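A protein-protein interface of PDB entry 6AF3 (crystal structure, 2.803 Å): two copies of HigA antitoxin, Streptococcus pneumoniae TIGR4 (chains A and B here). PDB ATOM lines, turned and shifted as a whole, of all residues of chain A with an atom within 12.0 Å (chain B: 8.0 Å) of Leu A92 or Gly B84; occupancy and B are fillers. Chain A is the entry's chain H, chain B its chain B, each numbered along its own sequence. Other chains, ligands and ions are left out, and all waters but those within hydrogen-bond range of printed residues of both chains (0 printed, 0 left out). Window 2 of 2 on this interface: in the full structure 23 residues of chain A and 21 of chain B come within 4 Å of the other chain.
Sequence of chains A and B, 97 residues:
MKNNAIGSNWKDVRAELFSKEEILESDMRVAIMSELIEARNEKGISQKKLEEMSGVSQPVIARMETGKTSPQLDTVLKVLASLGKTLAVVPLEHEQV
O of Ala B81 sits at hydrogen-bond distance from NZ of Lys A20 (2.7 Å).
The backbone carbonyl oxygen of Gly B84 sits close to the backbone NH of Leu A92 (3.5 Å).
N of Thr B86 lies within hydrogen-bond range of O of Val A90, at 3.0 Å.
N of Lys B85 is in hydrogen-bond range of O of Leu B80 (2.6 Å).
Leu A24 touches Leu B77.
Leu A24 touches Thr B86.
Val A89 touches Glu B35 (CG1 to OE2, 3.7 Å).
Val A89 touches Lys B85.
Val A89 touches Thr B86 (CG1 to O, 3.6 Å).
Val A90 touches Lys B85 (O to CA, 3.4 Å).
Printed residues of chain B within 4 Å of Lys A20: Ala B81 (2.7 Å).
Of the printed residues of chain B, Leu A24 touches Leu B77 (3.5 Å) and Thr B86 (3.4 Å).
Printed residues of chain B within 4 Å of Val A89: Glu B35 (3.7 Å), Lys B85 (3.6 Å) and Thr B86 (3.6 Å).
Leu A92 touches one residue of chain B.
Glu A93 touches none of the printed residues of chain B.
Of the printed residues of chain A, Glu B35 touches Val A89.
Lys B43 touches none of the printed residues of chain A.
No residue of chain A comes within 4 Å of Ser B82.
No residue of chain A comes within 4 Å of Leu B83.
Gly B84 touches just one residue of chain A: Leu A92 (3.0 Å).
Of the printed residues of chain A, Lys B85 touches Val A89 and Val A90.
The nearest residue of chain A that does not touch Gly B84 is Pro A91 (4.1 Å).
Of the 11 printed residues of chain A, 5 touch a printed residue of chain B.
Printed residues of chain A that touch a printed residue of chain B: Lys A20, Leu A24, Val A89, Val A90 and Leu A92.
Along chain A the printed residues that touch a printed residue of chain B span positions 20 to 92.
Of the 14 printed residues of chain B, 6 touch a printed residue of chain A.
Printed residues of chain B that touch a printed residue of chain A: Glu B35, Leu B77, Ala B81, Gly B84, Lys B85 and Thr B86.
Hydrophobic or aromatic side chains of chain B within 4 Å of the printed part of chain A: Leu B77 and Ala B81.
No position is printed for both chains.
Of the 9 pairs that touch across the chains among the printed residues, none has its exchanged pair printed and touching as well.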
ATOM      1  N   LYS A  20       4.101  -7.827 -22.645  1.00  0.00           N
ATOM      2  CA  LYS A  20       3.686  -8.269 -21.302  1.00  0.00           C
ATOM      3  C   LYS A  20       4.513  -7.556 -20.175  1.00  0.00           C
ATOM      4  O   LYS A  20       3.910  -7.067 -19.214  1.00  0.00           O
ATOM      5  CB  LYS A  20       3.759  -9.802 -21.213  1.00  0.00           C
ATOM      6  CG  LYS A  20       4.227 -10.381 -19.862  1.00  0.00           C
ATOM      7  CD  LYS A  20       4.585 -11.837 -20.039  1.00  0.00           C
ATOM      8  CE  LYS A  20       5.358 -12.408 -18.847  1.00  0.00           C
ATOM      9  NZ  LYS A  20       5.845 -13.821 -19.095  1.00  0.00           N
ATOM     10  N   GLU A  21       5.864  -7.572 -20.266  1.00  0.00           N
ATOM     11  CA  GLU A  21       6.812  -6.429 -20.025  1.00  0.00           C
ATOM     12  C   GLU A  21       6.286  -5.442 -18.905  1.00  0.00           C
ATOM     13  O   GLU A  21       6.086  -5.899 -17.777  1.00  0.00           O
ATOM     14  CB  GLU A  21       7.195  -5.829 -21.423  1.00  0.00           C
ATOM     15  CG  GLU A  21       7.933  -4.525 -21.601  1.00  0.00           C
ATOM     16  CD  GLU A  21       7.048  -3.546 -22.383  1.00  0.00           C
ATOM     17  OE1 GLU A  21       5.832  -3.759 -22.323  1.00  0.00           O
ATOM     18  OE2 GLU A  21       7.500  -2.546 -22.991  1.00  0.00           O
ATOM     19  N   ILE A  23       3.559  -3.446 -18.627  1.00  0.00           N
ATOM     20  CA  ILE A  23       2.104  -3.484 -18.433  1.00  0.00           C
ATOM     21  C   ILE A  23       1.763  -4.059 -17.058  1.00  0.00           C
ATOM     22  O   ILE A  23       0.887  -3.571 -16.346  1.00  0.00           O
ATOM     23  CB  ILE A  23       1.445  -4.351 -19.521  1.00  0.00           C
ATOM     24  CG1 ILE A  23       1.302  -3.554 -20.834  1.00  0.00           C
ATOM     25  CG2 ILE A  23       0.168  -5.022 -18.963  1.00  0.00           C
ATOM     26  CD1 ILE A  23       1.034  -4.422 -22.038  1.00  0.00           C
ATOM     27  N   LEU A  24       2.501  -5.098 -16.684  1.00  0.00           N
ATOM     28  CA  LEU A  24       2.319  -5.778 -15.420  1.00  0.00           C
ATOM     29  C   LEU A  24       2.790  -4.992 -14.231  1.00  0.00           C
ATOM     30  O   LEU A  24       2.332  -5.243 -13.122  1.00  0.00           O
ATOM     31  CB  LEU A  24       3.037  -7.094 -15.439  1.00  0.00           C
ATOM     32  CG  LEU A  24       2.510  -8.051 -16.473  1.00  0.00           C
ATOM     33  CD1 LEU A  24       2.860  -9.378 -15.939  1.00  0.00           C
ATOM     34  CD2 LEU A  24       0.973  -7.898 -16.731  1.00  0.00           C
ATOM     35  N   ASP A  27      -0.316  -2.266 -14.324  1.00  0.00           N
ATOM     36  CA  ASP A  27      -1.515  -2.930 -13.859  1.00  0.00           C
ATOM     37  C   ASP A  27      -1.547  -3.118 -12.361  1.00  0.00           C
ATOM     38  O   ASP A  27      -2.613  -3.214 -11.722  1.00  0.00           O
ATOM     39  CB  ASP A  27      -1.635  -4.274 -14.524  1.00  0.00           C
ATOM     40  CG  ASP A  27      -2.236  -4.183 -15.901  1.00  0.00           C
ATOM     41  OD1 ASP A  27      -2.309  -3.037 -16.432  1.00  0.00           O
ATOM     42  OD2 ASP A  27      -2.665  -5.236 -16.453  1.00  0.00           O
ATOM     43  N   ALA A  88      -2.310 -11.600  -3.556  1.00  0.00           N
ATOM     44  CA  ALA A  88      -2.392 -13.057  -3.601  1.00  0.00           C
ATOM     45  C   ALA A  88      -1.591 -13.430  -4.874  1.00  0.00           C
ATOM     46  O   ALA A  88      -1.437 -12.558  -5.731  1.00  0.00           O
ATOM     47  CB  ALA A  88      -3.759 -13.504  -3.673  1.00  0.00           C
ATOM     48  N   VAL A  89      -1.035 -14.650  -5.014  1.00  0.00           N
ATOM     49  CA  VAL A  89      -0.416 -14.993  -6.312  1.00  0.00           C
ATOM     50  C   VAL A  89      -1.349 -15.751  -7.208  1.00  0.00           C
ATOM     51  O   VAL A  89      -1.970 -16.715  -6.748  1.00  0.00           O
ATOM     52  CB  VAL A  89       0.841 -15.861  -6.174  1.00  0.00           C
ATOM     53  CG1 VAL A  89       1.479 -16.191  -7.591  1.00  0.00           C
ATOM     54  CG2 VAL A  89       1.815 -15.171  -5.365  1.00  0.00           C
ATOM     55  N   VAL A  90      -1.368 -15.391  -8.493  1.00  0.00           N
ATOM     56  CA  VAL A  90      -2.375 -15.875  -9.443  1.00  0.00           C
ATOM     57  C   VAL A  90      -1.789 -16.197 -10.797  1.00  0.00           C
ATOM     58  O   VAL A  90      -0.791 -15.618 -11.197  1.00  0.00           O
ATOM     59  CB  VAL A  90      -3.527 -14.833  -9.644  1.00  0.00           C
ATOM     60  CG1 VAL A  90      -4.213 -14.559  -8.312  1.00  0.00           C
ATOM     61  CG2 VAL A  90      -3.054 -13.497 -10.298  1.00  0.00           C
ATOM     62  N   PRO A  91      -2.358 -17.193 -11.476  1.00  0.00           N
ATOM     63  CA  PRO A  91      -1.906 -17.577 -12.817  1.00  0.00           C
ATOM     64  C   PRO A  91      -2.034 -16.564 -13.957  1.00  0.00           C
ATOM     65  O   PRO A  91      -2.617 -15.532 -13.757  1.00  0.00           O
ATOM     66  CB  PRO A  91      -2.743 -18.839 -13.080  1.00  0.00           C
ATOM     67  CG  PRO A  91      -2.779 -19.583 -11.644  1.00  0.00           C
ATOM     68  CD  PRO A  91      -2.765 -18.384 -10.655  1.00  0.00           C
ATOM     69  N   LEU A  92      -1.386 -16.866 -15.089  1.00  0.00           N
ATOM     70  CA  LEU A  92      -1.399 -16.184 -16.401  1.00  0.00           C
ATOM     71  C   LEU A  92      -2.717 -16.093 -17.203  1.00  0.00           C
ATOM     72  O   LEU A  92      -3.377 -17.108 -17.426  1.00  0.00           O
ATOM     73  CB  LEU A  92      -0.434 -16.918 -17.349  1.00  0.00           C
ATOM     74  CG  LEU A  92       0.914 -17.595 -17.038  1.00  0.00           C
ATOM     75  CD1 LEU A  92       0.711 -19.077 -16.584  1.00  0.00           C
ATOM     76  CD2 LEU A  92       1.908 -17.478 -18.232  1.00  0.00           C
ATOM     77  N   GLU A  93      -3.024 -14.897 -17.715  1.00  0.00           N
ATOM     78  CA  GLU A  93      -4.028 -14.679 -18.777  1.00  0.00           C
ATOM     79  C   GLU A  93      -5.440 -15.167 -18.400  1.00  0.00           C
ATOM     80  O   GLU A  93      -5.738 -16.365 -18.356  1.00  0.00           O
ATOM     81  CB  GLU A  93      -3.560 -15.342 -20.079  1.00  0.00           C
ATOM     82  CG  GLU A  93      -4.636 -15.618 -21.124  1.00  0.00           C
ATOM     83  CD  GLU A  93      -4.489 -17.018 -21.691  1.00  0.00           C
ATOM     84  OE1 GLU A  93      -3.375 -17.580 -21.532  1.00  0.00           O
ATOM     85  OE2 GLU A  93      -5.472 -17.559 -22.260  1.00  0.00           O
ATOM     86  N   GLU B  35       6.968 -20.602  -5.177  1.00  0.00           N
ATOM     87  CA  GLU B  35       7.012 -20.575  -6.625  1.00  0.00           C
ATOM     88  C   GLU B  35       8.423 -20.899  -7.076  1.00  0.00           C
ATOM     89  O   GLU B  35       8.590 -21.500  -8.134  1.00  0.00           O
ATOM     90  CB  GLU B  35       6.562 -19.223  -7.157  1.00  0.00           C
ATOM     91  CG  GLU B  35       5.153 -18.923  -6.773  1.00  0.00           C
ATOM     92  CD  GLU B  35       4.127 -19.474  -7.753  1.00  0.00           C
ATOM     93  OE1 GLU B  35       4.509 -19.747  -8.924  1.00  0.00           O
ATOM     94  OE2 GLU B  35       2.921 -19.636  -7.341  1.00  0.00           O
ATOM     95  N   LYS B  43       9.141 -27.460 -12.582  1.00  0.00           N
ATOM     96  CA  LYS B  43       9.367 -26.932 -13.933  1.00  0.00           C
ATOM     97  C   LYS B  43      10.811 -27.226 -14.416  1.00  0.00           C
ATOM     98  O   LYS B  43      10.986 -27.517 -15.596  1.00  0.00           O
ATOM     99  CB  LYS B  43       9.086 -25.417 -14.012  1.00  0.00           C
ATOM    100  CG  LYS B  43       7.605 -25.091 -14.008  1.00  0.00           C
ATOM    101  CD  LYS B  43       7.234 -23.640 -13.703  1.00  0.00           C
ATOM    102  CE  LYS B  43       5.747 -23.509 -13.667  1.00  0.00           C
ATOM    103  NZ  LYS B  43       5.293 -22.832 -12.378  1.00  0.00           N
ATOM    104  N   ILE B  45      13.695 -25.021 -13.746  1.00  0.00           N
ATOM    105  CA  ILE B  45      14.323 -23.833 -14.161  1.00  0.00           C
ATOM    106  C   ILE B  45      15.295 -23.532 -13.049  1.00  0.00           C
ATOM    107  O   ILE B  45      14.913 -23.285 -11.875  1.00  0.00           O
ATOM    108  CB  ILE B  45      13.267 -22.767 -14.456  1.00  0.00           C
ATOM    109  CG1 ILE B  45      12.665 -23.096 -15.789  1.00  0.00           C
ATOM    110  CG2 ILE B  45      13.807 -21.434 -14.557  1.00  0.00           C
ATOM    111  CD1 ILE B  45      11.362 -22.339 -15.997  1.00  0.00           C
ATOM    112  N   MET B  53      15.818 -14.812 -17.881  1.00  0.00           N
ATOM    113  CA  MET B  53      14.511 -14.639 -18.494  1.00  0.00           C
ATOM    114  C   MET B  53      13.840 -13.385 -17.971  1.00  0.00           C
ATOM    115  O   MET B  53      12.747 -13.034 -18.409  1.00  0.00           O
ATOM    116  CB  MET B  53      13.569 -15.802 -18.179  1.00  0.00           C
ATOM    117  CG  MET B  53      13.882 -17.139 -18.684  1.00  0.00           C
ATOM    118  SD  MET B  53      12.597 -18.490 -17.956  1.00  0.00           S
ATOM    119  CE  MET B  53      12.855 -18.040 -16.107  1.00  0.00           C
ATOM    120  N   LEU B  77       7.425  -8.970  -9.490  1.00  0.00           N
ATOM    121  CA  LEU B  77       6.636  -9.073 -10.712  1.00  0.00           C
ATOM    122  C   LEU B  77       7.462  -9.730 -11.848  1.00  0.00           C
ATOM    123  O   LEU B  77       6.996 -10.622 -12.579  1.00  0.00           O
ATOM    124  CB  LEU B  77       6.151  -7.679 -11.134  1.00  0.00           C
ATOM    125  CG  LEU B  77       5.264  -7.112 -10.043  1.00  0.00           C
ATOM    126  CD1 LEU B  77       4.566  -5.848 -10.505  1.00  0.00           C
ATOM    127  CD2 LEU B  77       4.277  -8.202  -9.601  1.00  0.00           C
ATOM    128  N   LYS B  78       8.679  -9.245 -11.979  1.00  0.00           N
ATOM    129  CA  LYS B  78       9.458  -9.619 -13.084  1.00  0.00           C
ATOM    130  C   LYS B  78       9.691 -11.131 -13.046  1.00  0.00           C
ATOM    131  O   LYS B  78       9.463 -11.861 -14.045  1.00  0.00           O
ATOM    132  CB  LYS B  78      10.790  -8.853 -13.049  1.00  0.00           C
ATOM    133  CG  LYS B  78      10.830  -7.680 -13.928  1.00  0.00           C
ATOM    134  CD  LYS B  78      11.957  -6.837 -13.500  1.00  0.00           C
ATOM    135  CE  LYS B  78      11.980  -5.522 -14.185  1.00  0.00           C
ATOM    136  NZ  LYS B  78      11.767  -4.601 -13.037  1.00  0.00           N
ATOM    137  N   VAL B  79      10.159 -11.558 -11.874  1.00  0.00           N
ATOM    138  CA  VAL B  79      10.384 -12.959 -11.528  1.00  0.00           C
ATOM    139  C   VAL B  79       9.131 -13.839 -11.675  1.00  0.00           C
ATOM    140  O   VAL B  79       9.165 -14.807 -12.452  1.00  0.00           O
ATOM    141  CB  VAL B  79      10.903 -13.134 -10.051  1.00  0.00           C
ATOM    142  CG1 VAL B  79      10.601 -14.599  -9.569  1.00  0.00           C
ATOM    143  CG2 VAL B  79      12.398 -12.673  -9.882  1.00  0.00           C
ATOM    144  N   LEU B  80       8.041 -13.502 -10.971  1.00  0.00           N
ATOM    145  CA  LEU B  80       6.828 -14.283 -11.099  1.00  0.00           C
ATOM    146  C   LEU B  80       6.412 -14.393 -12.569  1.00  0.00           C
ATOM    147  O   LEU B  80       5.932 -15.452 -13.050  1.00  0.00           O
ATOM    148  CB  LEU B  80       5.714 -13.676 -10.239  1.00  0.00           C
ATOM    149  CG  LEU B  80       6.035 -13.953  -8.758  1.00  0.00           C
ATOM    150  CD1 LEU B  80       5.181 -13.281  -7.707  1.00  0.00           C
ATOM    151  CD2 LEU B  80       6.034 -15.405  -8.572  1.00  0.00           C
ATOM    152  N   ALA B  81       6.633 -13.291 -13.290  1.00  0.00           N
ATOM    153  CA  ALA B  81       6.198 -13.174 -14.675  1.00  0.00           C
ATOM    154  C   ALA B  81       6.848 -14.183 -15.604  1.00  0.00           C
ATOM    155  O   ALA B  81       6.228 -14.615 -16.550  1.00  0.00           O
ATOM    156  CB  ALA B  81       6.445 -11.835 -15.153  1.00  0.00           C
ATOM    157  N   SER B  82       8.089 -14.549 -15.370  1.00  0.00           N
ATOM    158  CA  SER B  82       8.644 -15.640 -16.165  1.00  0.00           C
ATOM    159  C   SER B  82       8.260 -17.041 -15.597  1.00  0.00           C
ATOM    160  O   SER B  82       8.248 -18.061 -16.323  1.00  0.00           O
ATOM    161  CB  SER B  82      10.139 -15.495 -16.257  1.00  0.00           C
ATOM    162  OG  SER B  82      10.664 -14.922 -15.060  1.00  0.00           O
ATOM    163  N   LEU B  83       7.903 -17.070 -14.312  1.00  0.00           N
ATOM    164  CA  LEU B  83       7.379 -18.287 -13.674  1.00  0.00           C
ATOM    165  C   LEU B  83       5.879 -18.405 -13.970  1.00  0.00           C
ATOM    166  O   LEU B  83       5.198 -19.386 -13.590  1.00  0.00           O
ATOM    167  CB  LEU B  83       7.664 -18.266 -12.177  1.00  0.00           C
ATOM    168  CG  LEU B  83       9.074 -18.860 -12.026  1.00  0.00           C
ATOM    169  CD1 LEU B  83       9.527 -18.892 -10.547  1.00  0.00           C
ATOM    170  CD2 LEU B  83       9.228 -20.263 -12.787  1.00  0.00           C
ATOM    171  N   GLY B  84       5.435 -17.369 -14.706  1.00  0.00           N
ATOM    172  CA  GLY B  84       4.105 -17.253 -15.270  1.00  0.00           C
ATOM    173  C   GLY B  84       3.048 -16.912 -14.233  1.00  0.00           C
ATOM    174  O   GLY B  84       1.948 -17.492 -14.259  1.00  0.00           O
ATOM    175  N   LYS B  85       3.389 -16.031 -13.289  1.00  0.00           N
ATOM    176  CA  LYS B  85       2.432 -15.665 -12.270  1.00  0.00           C
ATOM    177  C   LYS B  85       2.439 -14.154 -12.078  1.00  0.00           C
ATOM    178  O   LYS B  85       3.425 -13.529 -12.336  1.00  0.00           O
ATOM    179  CB  LYS B  85       2.734 -16.375 -10.936  1.00  0.00           C
ATOM    180  CG  LYS B  85       2.971 -17.877 -10.975  1.00  0.00           C
ATOM    181  CD  LYS B  85       1.751 -18.667 -11.234  1.00  0.00           C
ATOM    182  CE  LYS B  85       2.116 -20.060 -10.949  1.00  0.00           C
ATOM    183  NZ  LYS B  85       0.921 -21.007 -11.000  1.00  0.00           N
ATOM    184  N   THR B  86       1.353 -13.530 -11.652  1.00  0.00           N
ATOM    185  CA  THR B  86       1.553 -12.175 -11.130  1.00  0.00           C
ATOM    186  C   THR B  86       1.059 -12.172  -9.769  1.00  0.00           C
ATOM    187  O   THR B  86       0.598 -13.187  -9.314  1.00  0.00           O
ATOM    188  CB  THR B  86       0.811 -10.970 -11.901  1.00  0.00           C
ATOM    189  OG1 THR B  86      -0.429 -11.390 -12.523  1.00  0.00           O
ATOM    190  CG2 THR B  86       1.762 -10.208 -12.869  1.00  0.00           C
